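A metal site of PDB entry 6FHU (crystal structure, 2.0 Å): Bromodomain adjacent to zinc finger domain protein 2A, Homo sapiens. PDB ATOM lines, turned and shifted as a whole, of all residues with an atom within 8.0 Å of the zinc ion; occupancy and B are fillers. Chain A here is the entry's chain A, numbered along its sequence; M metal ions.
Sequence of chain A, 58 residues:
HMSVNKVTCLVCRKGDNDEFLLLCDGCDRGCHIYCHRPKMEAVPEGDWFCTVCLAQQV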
ATOM      1  N   LEU A  10      20.350  -3.793  12.630  1.00  0.00           N
ATOM      2  CA  LEU A  10      21.322  -4.057  13.721  1.00  0.00           C
ATOM      3  C   LEU A  10      20.669  -4.314  15.080  1.00  0.00           C
ATOM      4  O   LEU A  10      21.191  -5.106  15.860  1.00  0.00           O
ATOM      5  CB  LEU A  10      22.286  -2.886  13.868  1.00  0.00           C
ATOM      6  CG  LEU A  10      23.291  -2.613  12.748  1.00  0.00           C
ATOM      7  CD1 LEU A  10      24.028  -1.289  12.950  1.00  0.00           C
ATOM      8  CD2 LEU A  10      24.292  -3.756  12.652  1.00  0.00           C
ATOM      9  N   LEU A  23      19.630   2.406   5.338  1.00  0.00           N
ATOM     10  CA  LEU A  23      20.846   1.771   4.860  1.00  0.00           C
ATOM     11  C   LEU A  23      22.014   2.727   5.125  1.00  0.00           C
ATOM     12  O   LEU A  23      21.921   3.929   4.813  1.00  0.00           O
ATOM     13  CB  LEU A  23      20.729   1.436   3.371  1.00  0.00           C
ATOM     14  CG  LEU A  23      19.418   0.772   2.903  1.00  0.00           C
ATOM     15  CD1 LEU A  23      19.418   0.486   1.395  1.00  0.00           C
ATOM     16  CD2 LEU A  23      19.146  -0.506   3.667  1.00  0.00           C
ATOM     17  N   CYS A  24      23.079   2.217   5.728  1.00  0.00           N
ATOM     18  CA  CYS A  24      24.233   3.039   6.099  1.00  0.00           C
ATOM     19  C   CYS A  24      24.985   3.499   4.845  1.00  0.00           C
ATOM     20  O   CYS A  24      25.264   2.684   3.978  1.00  0.00           O
ATOM     21  CB  CYS A  24      25.193   2.258   7.015  1.00  0.00           C
ATOM     22  SG  CYS A  24      26.687   3.176   7.471  1.00  0.00           S
ATOM     23  N   ASP A  25      25.331   4.789   4.792  1.00  0.00           N
ATOM     24  CA  ASP A  25      26.130   5.325   3.667  1.00  0.00           C
ATOM     25  C   ASP A  25      27.638   4.982   3.726  1.00  0.00           C
ATOM     26  O   ASP A  25      28.372   5.277   2.774  1.00  0.00           O
ATOM     27  CB  ASP A  25      25.930   6.846   3.532  1.00  0.00           C
ATOM     28  CG  ASP A  25      24.515   7.220   3.074  1.00  0.00           C
ATOM     29  OD1 ASP A  25      24.064   6.718   2.019  1.00  0.00           O
ATOM     30  OD2 ASP A  25      23.846   8.004   3.766  1.00  0.00           O
ATOM     31  N   GLY A  26      28.112   4.344   4.804  1.00  0.00           N
ATOM     32  CA  GLY A  26      29.507   3.911   4.913  1.00  0.00           C
ATOM     33  C   GLY A  26      29.788   2.409   4.841  1.00  0.00           C
ATOM     34  O   GLY A  26      30.966   2.018   4.742  1.00  0.00           O
ATOM     35  N   CYS A  27      28.750   1.572   4.892  1.00  0.00           N
ATOM     36  CA  CYS A  27      28.895   0.112   4.916  1.00  0.00           C
ATOM     37  C   CYS A  27      27.589  -0.525   4.472  1.00  0.00           C
ATOM     38  O   CYS A  27      26.671   0.170   4.028  1.00  0.00           O
ATOM     39  CB  CYS A  27      29.319  -0.352   6.322  1.00  0.00           C
ATOM     40  SG  CYS A  27      28.046  -0.379   7.629  1.00  0.00           S
ATOM     41  N   ASP A  28      27.468  -1.846   4.613  1.00  0.00           N
ATOM     42  CA  ASP A  28      26.251  -2.557   4.193  1.00  0.00           C
ATOM     43  C   ASP A  28      25.174  -2.744   5.297  1.00  0.00           C
ATOM     44  O   ASP A  28      24.212  -3.477   5.087  1.00  0.00           O
ATOM     45  CB  ASP A  28      26.626  -3.907   3.552  1.00  0.00           C
ATOM     46  CG  ASP A  28      27.158  -4.926   4.576  1.00  0.00           C
ATOM     47  OD1 ASP A  28      27.793  -4.528   5.599  1.00  0.00           O
ATOM     48  OD2 ASP A  28      26.944  -6.140   4.341  1.00  0.00           O
ATOM     49  N   ARG A  29      25.305  -2.037   6.423  1.00  0.00           N
ATOM     50  CA  ARG A  29      24.449  -2.270   7.599  1.00  0.00           C
ATOM     51  C   ARG A  29      23.178  -1.430   7.527  1.00  0.00           C
ATOM     52  O   ARG A  29      23.082  -0.492   6.728  1.00  0.00           O
ATOM     53  CB  ARG A  29      25.197  -1.972   8.884  1.00  0.00           C
ATOM     54  CG  ARG A  29      26.208  -3.045   9.287  1.00  0.00           C
ATOM     55  CD  ARG A  29      27.173  -2.513  10.343  1.00  0.00           C
ATOM     56  NE  ARG A  29      28.223  -3.473  10.659  1.00  0.00           N
ATOM     57  CZ  ARG A  29      29.428  -3.532  10.084  1.00  0.00           C
ATOM     58  NH1 ARG A  29      29.805  -2.658   9.148  1.00  0.00           N
ATOM     59  NH2 ARG A  29      30.279  -4.461  10.467  1.00  0.00           N
ATOM     60  N   GLY A  30      22.212  -1.751   8.383  1.00  0.00           N
ATOM     61  CA  GLY A  30      20.939  -1.046   8.409  1.00  0.00           C
ATOM     62  C   GLY A  30      20.293  -0.950   9.760  1.00  0.00           C
ATOM     63  O   GLY A  30      20.763  -1.576  10.725  1.00  0.00           O
ATOM     64  N   TRP A  48      23.260   9.069   6.474  1.00  0.00           N
ATOM     65  CA  TRP A  48      23.170   8.375   7.778  1.00  0.00           C
ATOM     66  C   TRP A  48      24.287   7.329   7.896  1.00  0.00           C
ATOM     67  O   TRP A  48      24.497   6.499   6.994  1.00  0.00           O
ATOM     68  CB  TRP A  48      21.791   7.738   7.999  1.00  0.00           C
ATOM     69  CG  TRP A  48      21.717   7.001   9.326  1.00  0.00           C
ATOM     70  CD1 TRP A  48      21.576   7.551  10.549  1.00  0.00           C
ATOM     71  CD2 TRP A  48      21.828   5.580   9.519  1.00  0.00           C
ATOM     72  NE1 TRP A  48      21.569   6.567  11.516  1.00  0.00           N
ATOM     73  CE2 TRP A  48      21.736   5.350  10.912  1.00  0.00           C
ATOM     74  CE3 TRP A  48      21.983   4.482   8.673  1.00  0.00           C
ATOM     75  CZ2 TRP A  48      21.819   4.065  11.464  1.00  0.00           C
ATOM     76  CZ3 TRP A  48      22.060   3.205   9.225  1.00  0.00           C
ATOM     77  CH2 TRP A  48      21.970   3.006  10.601  1.00  0.00           C
ATOM     78  N   PHE A  49      24.977   7.359   9.037  1.00  0.00           N
ATOM     79  CA  PHE A  49      26.053   6.434   9.356  1.00  0.00           C
ATOM     80  C   PHE A  49      25.705   5.623  10.576  1.00  0.00           C
ATOM     81  O   PHE A  49      25.321   6.178  11.602  1.00  0.00           O
ATOM     82  CB  PHE A  49      27.362   7.183   9.592  1.00  0.00           C
ATOM     83  CG  PHE A  49      27.900   7.817   8.345  1.00  0.00           C
ATOM     84  CD1 PHE A  49      28.591   7.047   7.412  1.00  0.00           C
ATOM     85  CD2 PHE A  49      27.672   9.163   8.061  1.00  0.00           C
ATOM     86  CE1 PHE A  49      29.079   7.614   6.237  1.00  0.00           C
ATOM     87  CE2 PHE A  49      28.149   9.732   6.894  1.00  0.00           C
ATOM     88  CZ  PHE A  49      28.840   8.961   5.976  1.00  0.00           C
ATOM     89  N   CYS A  50      25.840   4.308  10.453  1.00  0.00           N
ATOM     90  CA  CYS A  50      25.679   3.405  11.592  1.00  0.00           C
ATOM     91  C   CYS A  50      26.802   3.610  12.640  1.00  0.00           C
ATOM     92  O   CYS A  50      27.810   4.302  12.402  1.00  0.00           O
ATOM     93  CB  CYS A  50      25.651   1.945  11.137  1.00  0.00           C
ATOM     94  SG  CYS A  50      27.288   1.252  10.816  1.00  0.00           S
ATOM     95  N   THR A  51      26.616   2.975  13.797  1.00  0.00           N
ATOM     96  CA  THR A  51      27.522   3.111  14.937  1.00  0.00           C
ATOM     97  C   THR A  51      28.914   2.512  14.713  1.00  0.00           C
ATOM     98  O   THR A  51      29.897   2.937  15.335  1.00  0.00           O
ATOM     99  CB  THR A  51      26.879   2.481  16.181  1.00  0.00           C
ATOM    100  OG1 THR A  51      26.392   1.178  15.859  1.00  0.00           O
ATOM    101  CG2 THR A  51      25.716   3.338  16.641  1.00  0.00           C
ATOM    102  N   VAL A  52      29.005   1.525  13.818  1.00  0.00           N
ATOM    103  CA  VAL A  52      30.290   0.931  13.470  1.00  0.00           C
ATOM    104  C   VAL A  52      31.118   1.905  12.602  1.00  0.00           C
ATOM    105  O   VAL A  52      32.325   2.076  12.831  1.00  0.00           O
ATOM    106  CB  VAL A  52      30.114  -0.432  12.754  1.00  0.00           C
ATOM    107  CG1 VAL A  52      31.467  -1.017  12.376  1.00  0.00           C
ATOM    108  CG2 VAL A  52      29.304  -1.405  13.621  1.00  0.00           C
ATOM    109  N   CYS A  53      30.461   2.542  11.637  1.00  0.00           N
ATOM    110  CA  CYS A  53      31.100   3.631  10.867  1.00  0.00           C
ATOM    111  C   CYS A  53      31.442   4.865  11.727  1.00  0.00           C
ATOM    112  O   CYS A  53      32.518   5.462  11.540  1.00  0.00           O
ATOM    113  CB  CYS A  53      30.229   4.024   9.675  1.00  0.00           C
ATOM    114  SG  CYS A  53      30.133   2.732   8.401  1.00  0.00           S
ATOM    115  N   LEU A  54      30.570   5.224  12.667  1.00  0.00           N
ATOM    116  CA  LEU A  54      30.888   6.305  13.610  1.00  0.00           C
ATOM    117  C   LEU A  54      32.167   6.042  14.412  1.00  0.00           C
ATOM    118  O   LEU A  54      32.925   6.975  14.688  1.00  0.00           O
ATOM    119  CB  LEU A  54      29.744   6.555  14.596  1.00  0.00           C
ATOM    120  CG  LEU A  54      28.518   7.291  14.054  1.00  0.00           C
ATOM    121  CD1 LEU A  54      27.500   7.469  15.184  1.00  0.00           C
ATOM    122  CD2 LEU A  54      28.880   8.649  13.439  1.00  0.00           C
ATOM    123  N   GLN A  56      34.821   4.673  13.351  1.00  0.00           N
ATOM    124  CA  GLN A  56      35.985   4.915  12.478  1.00  0.00           C
ATOM    125  C   GLN A  56      36.301   6.405  12.250  1.00  0.00           C
ATOM    126  O   GLN A  56      37.384   6.735  11.747  1.00  0.00           O
ATOM    127  CB  GLN A  56      35.752   4.292  11.088  1.00  0.00           C
ATOM    128  CG  GLN A  56      35.552   2.794  11.069  1.00  0.00           C
ATOM    129  CD  GLN A  56      36.798   2.065  11.497  1.00  0.00           C
ATOM    130  OE1 GLN A  56      36.911   1.636  12.647  1.00  0.00           O
ATOM    131  NE2 GLN A  56      37.795   1.981  10.592  1.00  0.00           N
HETATM  132 ZN    ZN M   1      28.049   1.699   8.613  1.00  0.00          ZN
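The side-chain sulfur (SG) of Cys 27 lies close to the guanidinium group (NH1) of Arg 29, at 3.3 Å.
N of Gly 26 sits close to SG of Cys 24 (3.2 Å).
The backbone NH (N) of Cys 24 lies within hydrogen-bond range of the backbone carbonyl oxygen (O) of Arg 29 (2.9 Å).
The side-chain sulfur of Cys 50 sits close to the backbone NH of Val 52 (3.5 Å).
Of the 17 residues printed, 4 come within 4 Å of the zinc ion.
The nearest printed residue that does not touch the zinc ion is Gly 26 (4.2 Å).
The zinc ion is bound by SG of Cys 27 (2.3 Å).
SG of Cys 24 is bound to the zinc ion (2.3 Å).
The zinc ion is bound by the side-chain sulfur (SG) of Cys 53 (2.3 Å).
The zinc ion is bound by SG of Cys 50.
The zinc ion has four donor atoms within binding distance.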
